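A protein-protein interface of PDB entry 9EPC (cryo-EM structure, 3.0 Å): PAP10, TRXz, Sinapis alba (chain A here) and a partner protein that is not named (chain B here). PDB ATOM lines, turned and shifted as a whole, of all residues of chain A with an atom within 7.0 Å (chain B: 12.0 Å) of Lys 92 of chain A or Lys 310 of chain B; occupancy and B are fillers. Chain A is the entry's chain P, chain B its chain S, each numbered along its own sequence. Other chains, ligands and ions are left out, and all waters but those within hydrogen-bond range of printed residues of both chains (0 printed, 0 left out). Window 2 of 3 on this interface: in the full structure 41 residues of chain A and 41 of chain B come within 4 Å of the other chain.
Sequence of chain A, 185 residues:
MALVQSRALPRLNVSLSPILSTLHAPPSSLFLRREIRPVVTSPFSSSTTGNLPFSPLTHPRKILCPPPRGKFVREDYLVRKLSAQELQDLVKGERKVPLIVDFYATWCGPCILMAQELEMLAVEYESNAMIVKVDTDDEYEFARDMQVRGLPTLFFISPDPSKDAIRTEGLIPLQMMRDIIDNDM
The backbone carbonyl oxygen (O) of Val 91 of chain A lies within hydrogen-bond range of the side-chain amino group (NZ) of Lys 310 of chain B (3.1 Å). NZ of Lys 92 of chain A is in hydrogen-bond range of O of Gly 312 of chain B (3.2 Å). The guanidinium group (NH2) of Arg 95 of chain A lies close to the side-chain amino group (NZ) of Lys 310 of chain B (3.1 Å). The side-chain amino group of Lys 92 of chain A lies within hydrogen-bond range of the backbone carbonyl oxygen of Lys 310 of chain B (2.7 Å).
NH1 of Arg 95 of chain A is in hydrogen-bond range of O of Ser 158 of chain A, 2.7 Å away. The guanidinium group (NE) of Arg 95 of chain A is in hydrogen-bond range of the backbone carbonyl oxygen (O) of Leu 90 of chain A (2.8 Å). NH2 of Arg 95 of chain A sits at hydrogen-bond distance from O of Val 91 of chain A, 2.7 Å away.
Among the printed residues, merely in contact across the chains: Gln 88 of chain A with Leu 314 of chain B (3.97 Å), Val 91 of chain A with Leu 314 of chain B (3.7 Å) and Ile 157 of chain A with Ile 308 of chain B (3.7 Å).
Gln 88 of chain A touches just one residue of chain B: Leu 314 (3.97 Å). No residue of chain B comes within 4 Å of Asp 89 of chain A. Val 91 of chain A touches two residues of chain B. Of the printed residues of chain B, Lys 92 of chain A touches Lys 310 (2.7 Å) and Gly 312 (3.2 Å). Glu 94 of chain A touches none of the printed residues of chain B. Of the printed residues of chain B, Arg 95 of chain A touches Lys 310 (3.1 Å). Of the printed residues of chain B, Ile 157 of chain A touches Ile 308. No residue of chain B comes within 4 Å of Pro 161 of chain A. Printed residues of chain A within 4 Å of Ile 308 of chain B: Ile 157 (3.7 Å). Lys 310 of chain B touches three residues of chain A. Of the printed residues of chain A, Gly 312 of chain B touches Lys 92 (3.2 Å). Printed residues of chain A within 4 Å of Leu 314 of chain B: Gln 88 (3.97 Å) and Val 91 (3.7 Å). The nearest residue of chain B that does not touch Lys 92 of chain A is Arg 311 of chain B (4.1 Å). The nearest residue of chain A that does not touch Lys 310 of chain B is Pro 161 of chain A (4.7 Å).
Printed residues of chain A that touch a printed residue of chain B: Gln 88, Val 91, Lys 92, Arg 95 and Ile 157. Hydrophobic or aromatic side chains of chain A that line the printed part of chain B: Val 91 and Ile 157. Of the 12 printed residues of chain B, 4 touch a printed residue of chain A. Along chain B the printed residues that touch a printed residue of chain A span positions 308 to 314.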
ATOM      1  N   LEU A  87      -2.937  -1.203   5.904  1.00  0.00           N
ATOM      2  CA  LEU A  87      -2.864  -2.216   4.864  1.00  0.00           C
ATOM      3  C   LEU A  87      -4.166  -2.980   4.677  1.00  0.00           C
ATOM      4  O   LEU A  87      -4.363  -3.582   3.617  1.00  0.00           O
ATOM      5  CB  LEU A  87      -1.738  -3.208   5.176  1.00  0.00           C
ATOM      6  CG  LEU A  87      -1.208  -4.029   4.003  1.00  0.00           C
ATOM      7  CD1 LEU A  87      -0.580  -3.114   2.971  1.00  0.00           C
ATOM      8  CD2 LEU A  87      -0.209  -5.055   4.488  1.00  0.00           C
ATOM      9  N   GLN A  88      -5.057  -2.967   5.670  1.00  0.00           N
ATOM     10  CA  GLN A  88      -6.313  -3.701   5.548  1.00  0.00           C
ATOM     11  C   GLN A  88      -7.214  -3.066   4.498  1.00  0.00           C
ATOM     12  O   GLN A  88      -7.636  -3.726   3.543  1.00  0.00           O
ATOM     13  CB  GLN A  88      -7.020  -3.754   6.900  1.00  0.00           C
ATOM     14  CG  GLN A  88      -6.193  -4.371   8.000  1.00  0.00           C
ATOM     15  CD  GLN A  88      -6.877  -4.287   9.345  1.00  0.00           C
ATOM     16  OE1 GLN A  88      -7.994  -3.785   9.455  1.00  0.00           O
ATOM     17  NE2 GLN A  88      -6.212  -4.791  10.377  1.00  0.00           N
ATOM     18  N   ASP A  89      -7.517  -1.777   4.661  1.00  0.00           N
ATOM     19  CA  ASP A  89      -8.353  -1.086   3.687  1.00  0.00           C
ATOM     20  C   ASP A  89      -7.706  -1.083   2.311  1.00  0.00           C
ATOM     21  O   ASP A  89      -8.404  -0.997   1.296  1.00  0.00           O
ATOM     22  CB  ASP A  89      -8.628   0.349   4.142  1.00  0.00           C
ATOM     23  CG  ASP A  89      -9.818   0.967   3.434  1.00  0.00           C
ATOM     24  OD1 ASP A  89     -10.251   0.411   2.403  1.00  0.00           O
ATOM     25  OD2 ASP A  89     -10.383   2.007   3.833  1.00  0.00           O
ATOM     26  N   LEU A  90      -6.376  -1.182   2.255  1.00  0.00           N
ATOM     27  CA  LEU A  90      -5.703  -1.304   0.969  1.00  0.00           C
ATOM     28  C   LEU A  90      -6.072  -2.609   0.277  1.00  0.00           C
ATOM     29  O   LEU A  90      -6.270  -2.635  -0.943  1.00  0.00           O
ATOM     30  CB  LEU A  90      -4.190  -1.200   1.155  1.00  0.00           C
ATOM     31  CG  LEU A  90      -3.564   0.146   0.786  1.00  0.00           C
ATOM     32  CD1 LEU A  90      -3.625   0.367  -0.714  1.00  0.00           C
ATOM     33  CD2 LEU A  90      -4.258   1.280   1.518  1.00  0.00           C
ATOM     34  N   VAL A  91      -6.179  -3.700   1.034  1.00  0.00           N
ATOM     35  CA  VAL A  91      -6.475  -5.001   0.446  1.00  0.00           C
ATOM     36  C   VAL A  91      -7.971  -5.275   0.519  1.00  0.00           C
ATOM     37  O   VAL A  91      -8.517  -6.003  -0.316  1.00  0.00           O
ATOM     38  CB  VAL A  91      -5.666  -6.122   1.125  1.00  0.00           C
ATOM     39  CG1 VAL A  91      -4.179  -5.851   0.991  1.00  0.00           C
ATOM     40  CG2 VAL A  91      -6.053  -6.266   2.586  1.00  0.00           C
ATOM     41  N   LYS A  92      -8.647  -4.699   1.516  1.00  0.00           N
ATOM     42  CA  LYS A  92     -10.100  -4.817   1.571  1.00  0.00           C
ATOM     43  C   LYS A  92     -10.780  -3.905   0.563  1.00  0.00           C
ATOM     44  O   LYS A  92     -11.863  -4.235   0.065  1.00  0.00           O
ATOM     45  CB  LYS A  92     -10.610  -4.508   2.979  1.00  0.00           C
ATOM     46  CG  LYS A  92     -10.270  -5.569   4.007  1.00  0.00           C
ATOM     47  CD  LYS A  92     -10.877  -5.236   5.358  1.00  0.00           C
ATOM     48  CE  LYS A  92     -10.584  -6.323   6.375  1.00  0.00           C
ATOM     49  NZ  LYS A  92     -11.135  -7.639   5.953  1.00  0.00           N
ATOM     50  N   GLY A  93     -10.171  -2.768   0.253  1.00  0.00           N
ATOM     51  CA  GLY A  93     -10.716  -1.824  -0.700  1.00  0.00           C
ATOM     52  C   GLY A  93     -10.257  -2.103  -2.113  1.00  0.00           C
ATOM     53  O   GLY A  93      -9.930  -3.234  -2.484  1.00  0.00           O
ATOM     54  N   GLU A  94     -10.238  -1.044  -2.914  1.00  0.00           N
ATOM     55  CA  GLU A  94      -9.886  -1.163  -4.321  1.00  0.00           C
ATOM     56  C   GLU A  94      -8.374  -1.108  -4.506  1.00  0.00           C
ATOM     57  O   GLU A  94      -7.660  -0.405  -3.786  1.00  0.00           O
ATOM     58  CB  GLU A  94     -10.554  -0.047  -5.123  1.00  0.00           C
ATOM     59  CG  GLU A  94     -10.616  -0.284  -6.628  1.00  0.00           C
ATOM     60  CD  GLU A  94      -9.327   0.069  -7.344  1.00  0.00           C
ATOM     61  OE1 GLU A  94      -9.023  -0.562  -8.379  1.00  0.00           O
ATOM     62  OE2 GLU A  94      -8.621   0.984  -6.877  1.00  0.00           O
ATOM     63  N   ARG A  95      -7.892  -1.875  -5.478  1.00  0.00           N
ATOM     64  CA  ARG A  95      -6.488  -1.848  -5.876  1.00  0.00           C
ATOM     65  C   ARG A  95      -6.441  -1.842  -7.394  1.00  0.00           C
ATOM     66  O   ARG A  95      -6.808  -2.833  -8.029  1.00  0.00           O
ATOM     67  CB  ARG A  95      -5.722  -3.038  -5.307  1.00  0.00           C
ATOM     68  CG  ARG A  95      -5.054  -2.771  -3.978  1.00  0.00           C
ATOM     69  CD  ARG A  95      -4.642  -4.067  -3.310  1.00  0.00           C
ATOM     70  NE  ARG A  95      -5.789  -4.775  -2.757  1.00  0.00           N
ATOM     71  CZ  ARG A  95      -6.418  -5.778  -3.354  1.00  0.00           C
ATOM     72  NH1 ARG A  95      -6.033  -6.231  -4.536  1.00  0.00           N
ATOM     73  NH2 ARG A  95      -7.457  -6.344  -2.747  1.00  0.00           N
ATOM     74  N   ILE A 157       0.383  -8.334  -4.213  1.00  0.00           N
ATOM     75  CA  ILE A 157      -1.074  -8.361  -4.231  1.00  0.00           C
ATOM     76  C   ILE A 157      -1.541  -7.952  -5.618  1.00  0.00           C
ATOM     77  O   ILE A 157      -1.235  -6.848  -6.084  1.00  0.00           O
ATOM     78  CB  ILE A 157      -1.671  -7.440  -3.158  1.00  0.00           C
ATOM     79  CG1 ILE A 157      -1.243  -7.894  -1.765  1.00  0.00           C
ATOM     80  CG2 ILE A 157      -3.181  -7.429  -3.265  1.00  0.00           C
ATOM     81  CD1 ILE A 157      -1.872  -9.195  -1.332  1.00  0.00           C
ATOM     82  N   SER A 158      -2.282  -8.838  -6.271  1.00  0.00           N
ATOM     83  CA  SER A 158      -2.821  -8.527  -7.583  1.00  0.00           C
ATOM     84  C   SER A 158      -3.894  -7.448  -7.465  1.00  0.00           C
ATOM     85  O   SER A 158      -4.648  -7.426  -6.486  1.00  0.00           O
ATOM     86  CB  SER A 158      -3.411  -9.778  -8.229  1.00  0.00           C
ATOM     87  OG  SER A 158      -4.028  -9.469  -9.465  1.00  0.00           O
ATOM     88  N   ASP A 160      -6.543  -7.374  -9.212  1.00  0.00           N
ATOM     89  CA  ASP A 160      -7.785  -8.128  -9.283  1.00  0.00           C
ATOM     90  C   ASP A 160      -7.911  -9.025  -8.059  1.00  0.00           C
ATOM     91  O   ASP A 160      -7.043  -9.875  -7.836  1.00  0.00           O
ATOM     92  CB  ASP A 160      -7.823  -8.966 -10.554  1.00  0.00           C
ATOM     93  CG  ASP A 160      -9.118  -9.739 -10.709  1.00  0.00           C
ATOM     94  OD1 ASP A 160     -10.106  -9.406 -10.023  1.00  0.00           O
ATOM     95  OD2 ASP A 160      -9.147 -10.689 -11.519  1.00  0.00           O
ATOM     96  N   PRO A 161      -8.963  -8.878  -7.249  1.00  0.00           N
ATOM     97  CA  PRO A 161      -9.100  -9.739  -6.062  1.00  0.00           C
ATOM     98  C   PRO A 161      -9.254 -11.214  -6.387  1.00  0.00           C
ATOM     99  O   PRO A 161      -9.036 -12.049  -5.501  1.00  0.00           O
ATOM    100  CB  PRO A 161     -10.356  -9.188  -5.373  1.00  0.00           C
ATOM    101  CG  PRO A 161     -10.480  -7.786  -5.873  1.00  0.00           C
ATOM    102  CD  PRO A 161      -9.985  -7.819  -7.285  1.00  0.00           C
ATOM    103  N   LYS A 163      -7.423 -13.170  -8.364  1.00  0.00           N
ATOM    104  CA  LYS A 163      -6.151 -13.874  -8.367  1.00  0.00           C
ATOM    105  C   LYS A 163      -5.537 -13.905  -6.969  1.00  0.00           C
ATOM    106  O   LYS A 163      -5.783 -13.037  -6.127  1.00  0.00           O
ATOM    107  CB  LYS A 163      -5.180 -13.232  -9.358  1.00  0.00           C
ATOM    108  CG  LYS A 163      -5.367 -13.711 -10.787  1.00  0.00           C
ATOM    109  CD  LYS A 163      -4.357 -13.079 -11.726  1.00  0.00           C
ATOM    110  CE  LYS A 163      -4.575 -11.582 -11.838  1.00  0.00           C
ATOM    111  NZ  LYS A 163      -5.937 -11.245 -12.334  1.00  0.00           N
ATOM    112  N   MET B 306      -0.220 -17.114  -2.223  1.00  0.00           N
ATOM    113  CA  MET B 306      -0.968 -16.866  -1.001  1.00  0.00           C
ATOM    114  C   MET B 306      -2.406 -16.502  -1.331  1.00  0.00           C
ATOM    115  O   MET B 306      -2.675 -15.829  -2.330  1.00  0.00           O
ATOM    116  CB  MET B 306      -0.341 -15.738  -0.170  1.00  0.00           C
ATOM    117  CG  MET B 306       0.659 -16.217   0.861  1.00  0.00           C
ATOM    118  SD  MET B 306       0.096 -17.736   1.654  1.00  0.00           S
ATOM    119  CE  MET B 306       1.648 -18.590   1.918  1.00  0.00           C
ATOM    120  N   LYS B 307      -3.323 -16.947  -0.479  1.00  0.00           N
ATOM    121  CA  LYS B 307      -4.734 -16.593  -0.568  1.00  0.00           C
ATOM    122  C   LYS B 307      -5.037 -15.618   0.561  1.00  0.00           C
ATOM    123  O   LYS B 307      -5.061 -16.005   1.734  1.00  0.00           O
ATOM    124  CB  LYS B 307      -5.616 -17.834  -0.481  1.00  0.00           C
ATOM    125  CG  LYS B 307      -7.096 -17.537  -0.374  1.00  0.00           C
ATOM    126  CD  LYS B 307      -7.904 -18.821  -0.335  1.00  0.00           C
ATOM    127  CE  LYS B 307      -9.366 -18.537  -0.040  1.00  0.00           C
ATOM    128  NZ  LYS B 307      -9.541 -17.903   1.295  1.00  0.00           N
ATOM    129  N   ILE B 308      -5.263 -14.356   0.207  1.00  0.00           N
ATOM    130  CA  ILE B 308      -5.464 -13.297   1.188  1.00  0.00           C
ATOM    131  C   ILE B 308      -6.955 -13.237   1.502  1.00  0.00           C
ATOM    132  O   ILE B 308      -7.743 -12.676   0.740  1.00  0.00           O
ATOM    133  CB  ILE B 308      -4.941 -11.951   0.686  1.00  0.00           C
ATOM    134  CG1 ILE B 308      -3.439 -12.033   0.417  1.00  0.00           C
ATOM    135  CG2 ILE B 308      -5.224 -10.865   1.704  1.00  0.00           C
ATOM    136  CD1 ILE B 308      -2.625 -12.353   1.644  1.00  0.00           C
ATOM    137  N   SER B 309      -7.342 -13.823   2.629  1.00  0.00           N
ATOM    138  CA  SER B 309      -8.704 -13.664   3.114  1.00  0.00           C
ATOM    139  C   SER B 309      -8.912 -12.237   3.597  1.00  0.00           C
ATOM    140  O   SER B 309      -8.023 -11.637   4.206  1.00  0.00           O
ATOM    141  CB  SER B 309      -8.988 -14.651   4.244  1.00  0.00           C
ATOM    142  OG  SER B 309     -10.318 -14.515   4.712  1.00  0.00           O
ATOM    143  N   LYS B 310     -10.089 -11.680   3.306  1.00  0.00           N
ATOM    144  CA  LYS B 310     -10.400 -10.324   3.743  1.00  0.00           C
ATOM    145  C   LYS B 310     -11.848 -10.205   4.202  1.00  0.00           C
ATOM    146  O   LYS B 310     -12.446  -9.127   4.111  1.00  0.00           O
ATOM    147  CB  LYS B 310     -10.108  -9.313   2.632  1.00  0.00           C
ATOM    148  CG  LYS B 310     -10.847  -9.585   1.334  1.00  0.00           C
ATOM    149  CD  LYS B 310     -10.145  -8.934   0.154  1.00  0.00           C
ATOM    150  CE  LYS B 310      -8.751  -9.511  -0.040  1.00  0.00           C
ATOM    151  NZ  LYS B 310      -8.064  -8.932  -1.226  1.00  0.00           N
ATOM    152  N   ARG B 311     -12.424 -11.295   4.707  1.00  0.00           N
ATOM    153  CA  ARG B 311     -13.800 -11.258   5.191  1.00  0.00           C
ATOM    154  C   ARG B 311     -13.866 -10.700   6.610  1.00  0.00           C
ATOM    155  O   ARG B 311     -14.523  -9.684   6.860  1.00  0.00           O
ATOM    156  CB  ARG B 311     -14.416 -12.657   5.123  1.00  0.00           C
ATOM    157  CG  ARG B 311     -15.275 -12.901   3.889  1.00  0.00           C
ATOM    158  CD  ARG B 311     -14.586 -12.438   2.612  1.00  0.00           C
ATOM    159  NE  ARG B 311     -13.343 -13.157   2.355  1.00  0.00           N
ATOM    160  CZ  ARG B 311     -12.582 -12.976   1.286  1.00  0.00           C
ATOM    161  NH1 ARG B 311     -12.904 -12.100   0.347  1.00  0.00           N
ATOM    162  NH2 ARG B 311     -11.469 -13.690   1.153  1.00  0.00           N
ATOM    163  N   GLY B 312     -13.192 -11.357   7.550  1.00  0.00           N
ATOM    164  CA  GLY B 312     -13.125 -10.874   8.915  1.00  0.00           C
ATOM    165  C   GLY B 312     -11.802 -10.198   9.203  1.00  0.00           C
ATOM    166  O   GLY B 312     -11.580  -9.055   8.794  1.00  0.00           O
ATOM    167  N   ARG B 313     -10.915 -10.894   9.907  1.00  0.00           N
ATOM    168  CA  ARG B 313      -9.544 -10.435  10.074  1.00  0.00           C
ATOM    169  C   ARG B 313      -8.670 -11.122   9.035  1.00  0.00           C
ATOM    170  O   ARG B 313      -8.699 -12.349   8.904  1.00  0.00           O
ATOM    171  CB  ARG B 313      -9.030 -10.714  11.486  1.00  0.00           C
ATOM    172  CG  ARG B 313      -8.205  -9.583  12.095  1.00  0.00           C
ATOM    173  CD  ARG B 313      -7.772  -9.873  13.536  1.00  0.00           C
ATOM    174  NE  ARG B 313      -7.004  -8.782  14.126  1.00  0.00           N
ATOM    175  CZ  ARG B 313      -6.676  -8.701  15.409  1.00  0.00           C
ATOM    176  NH1 ARG B 313      -7.004  -9.652  16.268  1.00  0.00           N
ATOM    177  NH2 ARG B 313      -6.016  -7.632  15.843  1.00  0.00           N
ATOM    178  N   LEU B 314      -7.901 -10.327   8.295  1.00  0.00           N
ATOM    179  CA  LEU B 314      -7.204 -10.842   7.125  1.00  0.00           C
ATOM    180  C   LEU B 314      -6.117 -11.831   7.531  1.00  0.00           C
ATOM    181  O   LEU B 314      -5.327 -11.572   8.443  1.00  0.00           O
ATOM    182  CB  LEU B 314      -6.615  -9.694   6.302  1.00  0.00           C
ATOM    183  CG  LEU B 314      -5.337  -8.962   6.717  1.00  0.00           C
ATOM    184  CD1 LEU B 314      -4.954  -7.953   5.650  1.00  0.00           C
ATOM    185  CD2 LEU B 314      -5.483  -8.280   8.062  1.00  0.00           C
ATOM    186  N   LYS B 315      -6.093 -12.973   6.855  1.00  0.00           N
ATOM    187  CA  LYS B 315      -5.145 -14.046   7.099  1.00  0.00           C
ATOM    188  C   LYS B 315      -4.425 -14.385   5.799  1.00  0.00           C
ATOM    189  O   LYS B 315      -4.574 -13.705   4.782  1.00  0.00           O
ATOM    190  CB  LYS B 315      -5.849 -15.283   7.663  1.00  0.00           C
ATOM    191  CG  LYS B 315      -6.716 -15.017   8.877  1.00  0.00           C
ATOM    192  CD  LYS B 315      -5.914 -14.399  10.007  1.00  0.00           C
ATOM    193  CE  LYS B 315      -6.689 -14.445  11.312  1.00  0.00           C
ATOM    194  NZ  LYS B 315      -8.034 -13.825  11.176  1.00  0.00           N
ATOM    195  N   SER B 316      -3.635 -15.454   5.841  1.00  0.00           N
ATOM    196  CA  SER B 316      -2.931 -15.952   4.668  1.00  0.00           C
ATOM    197  C   SER B 316      -2.809 -17.462   4.775  1.00  0.00           C
ATOM    198  O   SER B 316      -2.254 -17.972   5.753  1.00  0.00           O
ATOM    199  CB  SER B 316      -1.549 -15.307   4.536  1.00  0.00           C
ATOM    200  OG  SER B 316      -1.660 -13.902   4.404  1.00  0.00           O
ATOM    201  N   THR B 317      -3.332 -18.171   3.781  1.00  0.00           N
ATOM    202  CA  THR B 317      -3.205 -19.618   3.693  1.00  0.00           C
ATOM    203  C   THR B 317      -2.400 -19.980   2.453  1.00  0.00           C
ATOM    204  O   THR B 317      -2.525 -19.332   1.408  1.00  0.00           O
ATOM    205  CB  THR B 317      -4.578 -20.299   3.654  1.00  0.00           C
ATOM    206  OG1 THR B 317      -4.411 -21.683   3.316  1.00  0.00           O
ATOM    207  CG2 THR B 317      -5.481 -19.630   2.634  1.00  0.00           C
